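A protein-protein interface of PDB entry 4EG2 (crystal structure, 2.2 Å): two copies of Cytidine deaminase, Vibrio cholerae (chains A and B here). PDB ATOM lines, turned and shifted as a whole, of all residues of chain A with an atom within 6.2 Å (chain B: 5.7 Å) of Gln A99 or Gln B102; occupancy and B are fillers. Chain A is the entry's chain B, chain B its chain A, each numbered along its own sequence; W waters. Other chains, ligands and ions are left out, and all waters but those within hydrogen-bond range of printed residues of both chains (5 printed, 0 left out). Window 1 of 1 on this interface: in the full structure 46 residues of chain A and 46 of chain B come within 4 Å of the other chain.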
ATOM      1  N   PHE A  95      -4.179 -21.218  -6.784  1.00  0.00           N
ATOM      2  CA  PHE A  95      -3.428 -22.457  -6.883  1.00  0.00           C
ATOM      3  C   PHE A  95      -4.299 -23.666  -6.789  1.00  0.00           C
ATOM      4  O   PHE A  95      -4.860 -23.948  -5.735  1.00  0.00           O
ATOM      5  CB  PHE A  95      -2.374 -22.496  -5.785  1.00  0.00           C
ATOM      6  CG  PHE A  95      -1.437 -21.348  -5.846  1.00  0.00           C
ATOM      7  CD1 PHE A  95      -0.385 -21.352  -6.753  1.00  0.00           C
ATOM      8  CD2 PHE A  95      -1.614 -20.240  -5.027  1.00  0.00           C
ATOM      9  CE1 PHE A  95       0.484 -20.274  -6.832  1.00  0.00           C
ATOM     10  CE2 PHE A  95      -0.737 -19.174  -5.094  1.00  0.00           C
ATOM     11  CZ  PHE A  95       0.305 -19.196  -6.009  1.00  0.00           C
ATOM     12  N   GLY A  97      -5.406 -27.320  -6.296  1.00  0.00           N
ATOM     13  CA  GLY A  97      -4.956 -28.354  -5.370  1.00  0.00           C
ATOM     14  C   GLY A  97      -4.539 -27.902  -3.978  1.00  0.00           C
ATOM     15  O   GLY A  97      -4.197 -28.759  -3.148  1.00  0.00           O
ATOM     16  N   ALA A  98      -4.579 -26.589  -3.717  1.00  0.00           N
ATOM     17  CA  ALA A  98      -4.176 -26.018  -2.432  1.00  0.00           C
ATOM     18  C   ALA A  98      -5.307 -25.285  -1.723  1.00  0.00           C
ATOM     19  O   ALA A  98      -6.194 -24.716  -2.359  1.00  0.00           O
ATOM     20  CB  ALA A  98      -3.005 -25.067  -2.627  1.00  0.00           C
ATOM     21  N   GLN A  99      -5.243 -25.249  -0.398  1.00  0.00           N
ATOM     22  CA  GLN A  99      -6.289 -24.592   0.386  1.00  0.00           C
ATOM     23  C   GLN A  99      -6.321 -23.084   0.005  1.00  0.00           C
ATOM     24  O   GLN A  99      -5.290 -22.494  -0.307  1.00  0.00           O
ATOM     25  CB  GLN A  99      -6.057 -24.837   1.875  1.00  0.00           C
ATOM     26  CG  GLN A  99      -7.309 -24.892   2.684  1.00  0.00           C
ATOM     27  CD  GLN A  99      -7.034 -25.152   4.143  1.00  0.00           C
ATOM     28  OE1 GLN A  99      -6.294 -24.403   4.790  1.00  0.00           O
ATOM     29  NE2 GLN A  99      -7.650 -26.191   4.682  1.00  0.00           N
ATOM     30  N   LEU A 100      -7.505 -22.473   0.040  1.00  0.00           N
ATOM     31  CA  LEU A 100      -7.682 -21.093  -0.461  1.00  0.00           C
ATOM     32  C   LEU A 100      -6.973 -19.959   0.288  1.00  0.00           C
ATOM     33  O   LEU A 100      -6.930 -18.823  -0.203  1.00  0.00           O
ATOM     34  CB  LEU A 100      -9.175 -20.779  -0.671  1.00  0.00           C
ATOM     35  CG  LEU A 100      -9.910 -21.599  -1.743  1.00  0.00           C
ATOM     36  CD1 LEU A 100     -11.336 -21.055  -1.955  1.00  0.00           C
ATOM     37  CD2 LEU A 100      -9.154 -21.598  -3.093  1.00  0.00           C
ATOM     38  N   GLY A 101      -6.418 -20.249   1.467  1.00  0.00           N
ATOM     39  CA  GLY A 101      -5.627 -19.268   2.184  1.00  0.00           C
ATOM     40  C   GLY A 101      -4.357 -18.934   1.397  1.00  0.00           C
ATOM     41  O   GLY A 101      -3.685 -17.933   1.662  1.00  0.00           O
ATOM     42  N   GLN A 102      -4.035 -19.756   0.403  1.00  0.00           N
ATOM     43  CA  GLN A 102      -2.858 -19.529  -0.434  1.00  0.00           C
ATOM     44  C   GLN A 102      -3.139 -18.549  -1.581  1.00  0.00           C
ATOM     45  O   GLN A 102      -2.234 -18.169  -2.312  1.00  0.00           O
ATOM     46  CB  GLN A 102      -2.347 -20.866  -0.986  1.00  0.00           C
ATOM     47  CG  GLN A 102      -1.990 -21.888   0.094  1.00  0.00           C
ATOM     48  CD  GLN A 102      -0.824 -21.438   0.959  1.00  0.00           C
ATOM     49  OE1 GLN A 102       0.288 -21.199   0.453  1.00  0.00           O
ATOM     50  NE2 GLN A 102      -1.048 -21.375   2.283  1.00  0.00           N
ATOM     51  N   THR A 103      -4.382 -18.123  -1.727  1.00  0.00           N
ATOM     52  CA  THR A 103      -4.741 -17.216  -2.812  1.00  0.00           C
ATOM     53  C   THR A 103      -4.133 -15.834  -2.596  1.00  0.00           C
ATOM     54  O   THR A 103      -3.894 -15.435  -1.468  1.00  0.00           O
ATOM     55  CB  THR A 103      -6.265 -17.069  -2.910  1.00  0.00           C
ATOM     56  OG1 THR A 103      -6.873 -18.371  -2.963  1.00  0.00           O
ATOM     57  CG2 THR A 103      -6.664 -16.240  -4.135  1.00  0.00           C
ATOM     58  N   ASN A 238      -5.724 -13.844   9.246  1.00  0.00           N
ATOM     59  CA  ASN A 238      -5.962 -14.501   7.949  1.00  0.00           C
ATOM     60  C   ASN A 238      -5.490 -13.709   6.725  1.00  0.00           C
ATOM     61  O   ASN A 238      -4.919 -14.296   5.812  1.00  0.00           O
ATOM     62  CB  ASN A 238      -7.409 -14.943   7.813  1.00  0.00           C
ATOM     63  CG  ASN A 238      -7.847 -15.778   8.989  1.00  0.00           C
ATOM     64  OD1 ASN A 238      -7.890 -15.272  10.114  1.00  0.00           O
ATOM     65  ND2 ASN A 238      -8.163 -17.051   8.754  1.00  0.00           N
ATOM     66  N   ASP A 279       3.130 -25.153   4.742  1.00  0.00           N
ATOM     67  CA  ASP A 279       2.413 -24.541   3.623  1.00  0.00           C
ATOM     68  C   ASP A 279       3.299 -24.190   2.434  1.00  0.00           C
ATOM     69  O   ASP A 279       2.821 -24.142   1.282  1.00  0.00           O
ATOM     70  CB  ASP A 279       1.589 -23.335   4.078  1.00  0.00           C
ATOM     71  CG  ASP A 279       0.233 -23.740   4.634  1.00  0.00           C
ATOM     72  OD1 ASP A 279      -0.538 -24.357   3.860  1.00  0.00           O
ATOM     73  OD2 ASP A 279      -0.076 -23.419   5.821  1.00  0.00           O
ATOM     74  N   MET B  93     -10.080 -18.861  17.656  1.00  0.00           N
ATOM     75  CA  MET B  93      -9.138 -19.983  17.847  1.00  0.00           C
ATOM     76  C   MET B  93      -7.895 -19.730  17.007  1.00  0.00           C
ATOM     77  O   MET B  93      -8.001 -19.397  15.822  1.00  0.00           O
ATOM     78  CB  MET B  93      -9.719 -21.318  17.406  1.00  0.00           C
ATOM     79  CG  MET B  93     -11.085 -21.601  17.917  1.00  0.00           C
ATOM     80  SD  MET B  93     -11.732 -23.392  17.404  1.00  0.00           S
ATOM     81  CE  MET B  93     -11.364 -23.417  15.493  1.00  0.00           C
ATOM     82  N   PHE B  95      -3.749 -21.245  16.189  1.00  0.00           N
ATOM     83  CA  PHE B  95      -2.944 -22.452  16.210  1.00  0.00           C
ATOM     84  C   PHE B  95      -1.476 -22.185  16.088  1.00  0.00           C
ATOM     85  O   PHE B  95      -0.978 -21.917  14.991  1.00  0.00           O
ATOM     86  CB  PHE B  95      -3.429 -23.388  15.106  1.00  0.00           C
ATOM     87  CG  PHE B  95      -4.826 -23.802  15.304  1.00  0.00           C
ATOM     88  CD1 PHE B  95      -5.121 -24.810  16.191  1.00  0.00           C
ATOM     89  CD2 PHE B  95      -5.874 -23.111  14.688  1.00  0.00           C
ATOM     90  CE1 PHE B  95      -6.443 -25.165  16.436  1.00  0.00           C
ATOM     91  CE2 PHE B  95      -7.191 -23.451  14.941  1.00  0.00           C
ATOM     92  CZ  PHE B  95      -7.477 -24.485  15.800  1.00  0.00           C
ATOM     93  N   ALA B  98       1.265 -23.023  13.124  1.00  0.00           N
ATOM     94  CA  ALA B  98       0.572 -23.151  11.818  1.00  0.00           C
ATOM     95  C   ALA B  98       0.432 -21.791  11.152  1.00  0.00           C
ATOM     96  O   ALA B  98       0.392 -20.762  11.830  1.00  0.00           O
ATOM     97  CB  ALA B  98      -0.779 -23.769  11.984  1.00  0.00           C
ATOM     98  N   GLN B  99       0.312 -21.783   9.824  1.00  0.00           N
ATOM     99  CA  GLN B  99       0.188 -20.524   9.098  1.00  0.00           C
ATOM    100  C   GLN B  99      -1.122 -19.846   9.523  1.00  0.00           C
ATOM    101  O   GLN B  99      -2.071 -20.525   9.858  1.00  0.00           O
ATOM    102  CB  GLN B  99       0.247 -20.764   7.601  1.00  0.00           C
ATOM    103  CG  GLN B  99       0.894 -19.644   6.822  1.00  0.00           C
ATOM    104  CD  GLN B  99       1.025 -19.990   5.345  1.00  0.00           C
ATOM    105  OE1 GLN B  99       0.031 -20.282   4.689  1.00  0.00           O
ATOM    106  NE2 GLN B  99       2.252 -19.939   4.819  1.00  0.00           N
ATOM    107  N   LEU B 100      -1.175 -18.515   9.485  1.00  0.00           N
ATOM    108  CA  LEU B 100      -2.345 -17.777   9.991  1.00  0.00           C
ATOM    109  C   LEU B 100      -3.678 -17.960   9.240  1.00  0.00           C
ATOM    110  O   LEU B 100      -4.713 -17.517   9.720  1.00  0.00           O
ATOM    111  CB  LEU B 100      -2.009 -16.290  10.232  1.00  0.00           C
ATOM    112  CG  LEU B 100      -0.940 -16.034  11.311  1.00  0.00           C
ATOM    113  CD1 LEU B 100      -0.715 -14.514  11.539  1.00  0.00           C
ATOM    114  CD2 LEU B 100      -1.303 -16.719  12.649  1.00  0.00           C
ATOM    115  N   GLY B 101      -3.656 -18.609   8.082  1.00  0.00           N
ATOM    116  CA  GLY B 101      -4.882 -18.932   7.363  1.00  0.00           C
ATOM    117  C   GLY B 101      -5.658 -20.007   8.121  1.00  0.00           C
ATOM    118  O   GLY B 101      -6.812 -20.269   7.825  1.00  0.00           O
ATOM    119  N   GLN B 102      -5.027 -20.630   9.115  1.00  0.00           N
ATOM    120  CA  GLN B 102      -5.699 -21.641   9.929  1.00  0.00           C
ATOM    121  C   GLN B 102      -6.464 -21.026  11.096  1.00  0.00           C
ATOM    122  O   GLN B 102      -7.150 -21.737  11.820  1.00  0.00           O
ATOM    123  CB  GLN B 102      -4.687 -22.663  10.453  1.00  0.00           C
ATOM    124  CG  GLN B 102      -3.924 -23.362   9.327  1.00  0.00           C
ATOM    125  CD  GLN B 102      -4.866 -24.113   8.397  1.00  0.00           C
ATOM    126  OE1 GLN B 102      -5.540 -25.050   8.809  1.00  0.00           O
ATOM    127  NE2 GLN B 102      -4.883 -23.724   7.133  1.00  0.00           N
ATOM    128  N   THR B 103      -6.355 -19.707  11.268  1.00  0.00           N
ATOM    129  CA  THR B 103      -7.032 -18.990  12.377  1.00  0.00           C
ATOM    130  C   THR B 103      -8.541 -18.940  12.186  1.00  0.00           C
ATOM    131  O   THR B 103      -9.018 -18.828  11.060  1.00  0.00           O
ATOM    132  CB  THR B 103      -6.522 -17.527  12.485  1.00  0.00           C
ATOM    133  OG1 THR B 103      -5.083 -17.514  12.546  1.00  0.00           O
ATOM    134  CG2 THR B 103      -7.113 -16.799  13.721  1.00  0.00           C
ATOM    135  N   VAL B 104      -9.292 -19.046  13.287  1.00  0.00           N
ATOM    136  CA  VAL B 104     -10.745 -18.925  13.232  1.00  0.00           C
ATOM    137  C   VAL B 104     -11.168 -17.748  14.103  1.00  0.00           C
ATOM    138  O   VAL B 104     -10.776 -17.641  15.251  1.00  0.00           O
ATOM    139  CB  VAL B 104     -11.476 -20.221  13.646  1.00  0.00           C
ATOM    140  CG1 VAL B 104     -12.996 -20.024  13.649  1.00  0.00           C
ATOM    141  CG2 VAL B 104     -11.096 -21.357  12.700  1.00  0.00           C
ATOM    142  N   PRO B 242     -12.158 -23.787   6.358  1.00  0.00           N
ATOM    143  CA  PRO B 242     -11.984 -25.220   6.077  1.00  0.00           C
ATOM    144  C   PRO B 242     -12.775 -26.106   7.050  1.00  0.00           C
ATOM    145  O   PRO B 242     -13.061 -25.685   8.144  1.00  0.00           O
ATOM    146  CB  PRO B 242     -10.464 -25.452   6.224  1.00  0.00           C
ATOM    147  CG  PRO B 242      -9.833 -24.104   6.295  1.00  0.00           C
ATOM    148  CD  PRO B 242     -10.882 -23.059   6.498  1.00  0.00           C
ATOM    149  N   PRO B 243     -13.098 -27.344   6.644  1.00  0.00           N
ATOM    150  CA  PRO B 243     -13.886 -28.267   7.471  1.00  0.00           C
ATOM    151  C   PRO B 243     -13.265 -28.611   8.818  1.00  0.00           C
ATOM    152  O   PRO B 243     -13.996 -28.782   9.789  1.00  0.00           O
ATOM    153  CB  PRO B 243     -13.997 -29.525   6.594  1.00  0.00           C
ATOM    154  CG  PRO B 243     -12.809 -29.446   5.678  1.00  0.00           C
ATOM    155  CD  PRO B 243     -12.609 -27.989   5.414  1.00  0.00           C
ATOM    156  N   LEU B 244     -11.947 -28.756   8.887  1.00  0.00           N
ATOM    157  CA  LEU B 244     -11.291 -29.056  10.185  1.00  0.00           C
ATOM    158  C   LEU B 244     -11.628 -27.951  11.176  1.00  0.00           C
ATOM    159  O   LEU B 244     -12.146 -28.202  12.251  1.00  0.00           O
ATOM    160  CB  LEU B 244      -9.771 -29.170  10.049  1.00  0.00           C
ATOM    161  CG  LEU B 244      -8.993 -29.382  11.373  1.00  0.00           C
ATOM    162  CD1 LEU B 244      -9.462 -30.641  12.136  1.00  0.00           C
ATOM    163  CD2 LEU B 244      -7.519 -29.442  11.125  1.00  0.00           C
ATOM    164  N   GLN B 245     -11.335 -26.722  10.782  1.00  0.00           N
ATOM    165  CA  GLN B 245     -11.622 -25.571  11.605  1.00  0.00           C
ATOM    166  C   GLN B 245     -13.053 -25.612  12.094  1.00  0.00           C
ATOM    167  O   GLN B 245     -13.313 -25.270  13.235  1.00  0.00           O
ATOM    168  CB  GLN B 245     -11.390 -24.263  10.840  1.00  0.00           C
ATOM    169  CG  GLN B 245      -9.978 -23.703  10.942  1.00  0.00           C
ATOM    170  CD  GLN B 245      -8.941 -24.552  10.282  1.00  0.00           C
ATOM    171  OE1 GLN B 245      -9.246 -25.391   9.417  1.00  0.00           O
ATOM    172  NE2 GLN B 245      -7.688 -24.352  10.687  1.00  0.00           N
ATOM    173  N   ILE B 274      -9.530 -27.931  -5.285  1.00  0.00           N
ATOM    174  CA  ILE B 274      -8.561 -27.832  -4.206  1.00  0.00           C
ATOM    175  C   ILE B 274      -8.664 -29.072  -3.307  1.00  0.00           C
ATOM    176  O   ILE B 274      -9.582 -29.890  -3.446  1.00  0.00           O
ATOM    177  CB  ILE B 274      -8.768 -26.594  -3.312  1.00  0.00           C
ATOM    178  CG1 ILE B 274     -10.166 -26.641  -2.666  1.00  0.00           C
ATOM    179  CG2 ILE B 274      -8.529 -25.311  -4.098  1.00  0.00           C
ATOM    180  CD1 ILE B 274     -10.356 -25.687  -1.469  1.00  0.00           C
ATOM    181  N   SER B 275      -7.715 -29.171  -2.381  1.00  0.00           N
ATOM    182  CA  SER B 275      -7.674 -30.216  -1.383  1.00  0.00           C
ATOM    183  C   SER B 275      -7.301 -29.611  -0.040  1.00  0.00           C
ATOM    184  O   SER B 275      -6.428 -28.743   0.033  1.00  0.00           O
ATOM    185  CB  SER B 275      -6.649 -31.283  -1.751  1.00  0.00           C
ATOM    186  OG  SER B 275      -6.529 -32.225  -0.709  1.00  0.00           O
ATOM    187  N   HIS B 276      -7.966 -30.083   1.014  1.00  0.00           N
ATOM    188  CA  HIS B 276      -7.691 -29.657   2.377  1.00  0.00           C
ATOM    189  C   HIS B 276      -6.755 -30.620   3.094  1.00  0.00           C
ATOM    190  O   HIS B 276      -6.420 -30.389   4.255  1.00  0.00           O
ATOM    191  CB  HIS B 276      -8.983 -29.641   3.191  1.00  0.00           C
ATOM    192  CG  HIS B 276      -9.984 -28.646   2.723  1.00  0.00           C
ATOM    193  ND1 HIS B 276      -9.757 -27.290   2.781  1.00  0.00           N
ATOM    194  CD2 HIS B 276     -11.236 -28.803   2.238  1.00  0.00           C
ATOM    195  CE1 HIS B 276     -10.817 -26.654   2.320  1.00  0.00           C
ATOM    196  NE2 HIS B 276     -11.731 -27.550   1.988  1.00  0.00           N
ATOM    197  N   ASP B 279      -3.240 -29.197   4.615  1.00  0.00           N
ATOM    198  CA  ASP B 279      -3.487 -28.292   5.741  1.00  0.00           C
ATOM    199  C   ASP B 279      -4.181 -28.957   6.929  1.00  0.00           C
ATOM    200  O   ASP B 279      -3.944 -28.579   8.084  1.00  0.00           O
ATOM    201  CB  ASP B 279      -4.225 -27.043   5.268  1.00  0.00           C
ATOM    202  CG  ASP B 279      -3.261 -25.969   4.745  1.00  0.00           C
ATOM    203  OD1 ASP B 279      -2.290 -25.638   5.479  1.00  0.00           O
ATOM    204  OD2 ASP B 279      -3.478 -25.435   3.630  1.00  0.00           O
ATOM    205  N   THR B 280      -5.024 -29.953   6.662  1.00  0.00           N
ATOM    206  CA  THR B 280      -5.648 -30.707   7.741  1.00  0.00           C
ATOM    207  C   THR B 280      -4.547 -31.503   8.468  1.00  0.00           C
ATOM    208  O   THR B 280      -4.515 -31.539   9.702  1.00  0.00           O
ATOM    209  CB  THR B 280      -6.731 -31.658   7.236  1.00  0.00           C
ATOM    210  OG1 THR B 280      -7.768 -30.913   6.579  1.00  0.00           O
ATOM    211  CG2 THR B 280      -7.322 -32.449   8.383  1.00  0.00           C
ATOM    212  N   THR B 283      -2.170 -28.919  10.437  1.00  0.00           N
ATOM    213  CA  THR B 283      -2.785 -28.344  11.616  1.00  0.00           C
ATOM    214  C   THR B 283      -2.991 -29.395  12.702  1.00  0.00           C
ATOM    215  O   THR B 283      -2.802 -29.103  13.878  1.00  0.00           O
ATOM    216  CB  THR B 283      -4.098 -27.642  11.257  1.00  0.00           C
ATOM    217  OG1 THR B 283      -3.821 -26.569  10.325  1.00  0.00           O
ATOM    218  CG2 THR B 283      -4.759 -27.086  12.486  1.00  0.00           C
HETATM  219  O   HOH W   1      -0.388 -27.272   4.333  1.00  0.00           O
HETATM  220  O   HOH W   2       0.530 -24.631   8.579  1.00  0.00           O
HETATM  221  O   HOH W   3      -2.939 -26.506   0.591  1.00  0.00           O
HETATM  222  O   HOH W   4       2.533 -20.028   1.746  1.00  0.00           O
HETATM  223  O   HOH W   5      -7.569 -26.608   7.719  1.00  0.00           O
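The side-chain amide oxygen (OE1) of Gln B99 lies within hydrogen-bond range of the side-chain amide nitrogen (NE2) of Gln A102, at 2.9 Å. OE1 of Gln B99 lies close to OD2 of Asp A279 (3.3 Å). OE1 of Gln A99 is in hydrogen-bond range of NE2 of Gln B102 (2.8 Å). ND2 of Asn A238 lies within hydrogen-bond range of O of Thr B103 (3.0 Å). NE2 of Gln A99 is in hydrogen-bond range of ND1 of His B276 (3.0 Å). OE1 of Gln A99 lies close to OD2 of Asp B279. The side-chain carboxylate of Asp B279 lies close to the side-chain carboxylate of Asp A279 (2.7 Å).
The side-chain hydroxyl (OG1) of Thr B103 sits at hydrogen-bond distance from the backbone carbonyl oxygen (O) of Leu B100 (2.9 Å). OG1 of Thr B283 lies within hydrogen-bond range of OE1 of Gln B102. The side-chain hydroxyl (OG1) of Thr B280 is in hydrogen-bond range of the backbone carbonyl oxygen (O) of His B276 (2.7 Å). The backbone carbonyl oxygen (O) of Asp B279 sits at hydrogen-bond distance from the side-chain hydroxyl (OG1) of Thr B283 (3.0 Å). The backbone carbonyl oxygen (O) of Leu A100 is in hydrogen-bond range of the side-chain hydroxyl (OG1) of Thr A103 (2.8 Å). NE2 of Gln A102 sits at hydrogen-bond distance from OD1 of Asp A279 (3.4 Å).
Among the printed residues, pairs that only touch across the chains: Gly A97 with Ile B274 (3.8 Å), Gly A97 with Ser B275 (3.6 Å), Ala A98 with Ile B274 (3.0 Å), Gln A99 with Pro B242 (3.3 Å), Gln A99 with Ser B275 (3.7 Å), Leu A100 with Ile B274 (3.9 Å), Asn A238 with Leu B100 (3.6 Å) and Asn A238 with Gly B101 (3.6 Å).
Gln A99 touches just these residues of chain B: Gln B102 (2.8 Å), Pro B242 (3.3 Å), Ser B275 (3.7 Å), His B276 (3.0 Å) and Asp B279 (3.2 Å). Of the printed residues of chain B, Asp A279 touches Gln B99 and Asp B279. Of the printed residues of chain A, Gly B101 touches Asn A238. Gln B102 touches just one residue of chain A: Gln A99 (2.8 Å). Of the printed residues of chain A, Thr B103 touches Asn A238 (3.0 Å). Printed residues of chain A within 4 Å of Ile B274: Gly A97, Ala A98 and Leu A100. Thr B280 touches none of the printed residues of chain A. Thr B283 touches none of the printed residues of chain A. The nearest printed residue of chain A that does not touch Asp B279 is Gln A102 (4.9 Å).
Along chain B the printed residues that touch a printed residue of chain A span positions 99 to 279. Of the 10 printed residues of chain A, 7 touch a printed residue of chain B. Hydrophobic or aromatic side chains of chain A that line the printed part of chain B: Leu A100. Among the printed residues, 15 pairs touch across the chains.
Gln A99 touches Gln B102, and with the chains exchanged Gln A102 touches Gln B99. Gln A99 touches Asp B279, and with the chains exchanged Asp A279 touches Gln B99. Asp A279 touches its own counterpart, Asp B279. Positions printed for both chains: 95, 98, 99, 100, 101, 102, 103 and 279. Of the 15 pairs that touch across the chains among the printed residues, 5 have their exchanged pair printed and touching as well.
Water W5 lies within hydrogen-bond range of the side-chain amide oxygen (OE1) of Gln B245 (2.7 Å), the side-chain amide oxygen (OE1) of Gln B102 (2.8 Å) and the side-chain amide nitrogen (NE2) of Gln A99 (3.1 Å). Water W1 bridges OD1 of Asp B279 (2.8 Å) and OD1 of Asp A279 (3.0 Å). Water W3 lies within hydrogen-bond range of N of Gln A99 and OD2 of Asp B279. Water W4 bridges OE1 of Gln A102 (2.8 Å) and NE2 of Gln B99 (3.1 Å). Water W2 lies within hydrogen-bond range of the side-chain carboxylate of Asp A279 (3.1 Å) and the backbone NH of Gln B99 (3.1 Å).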
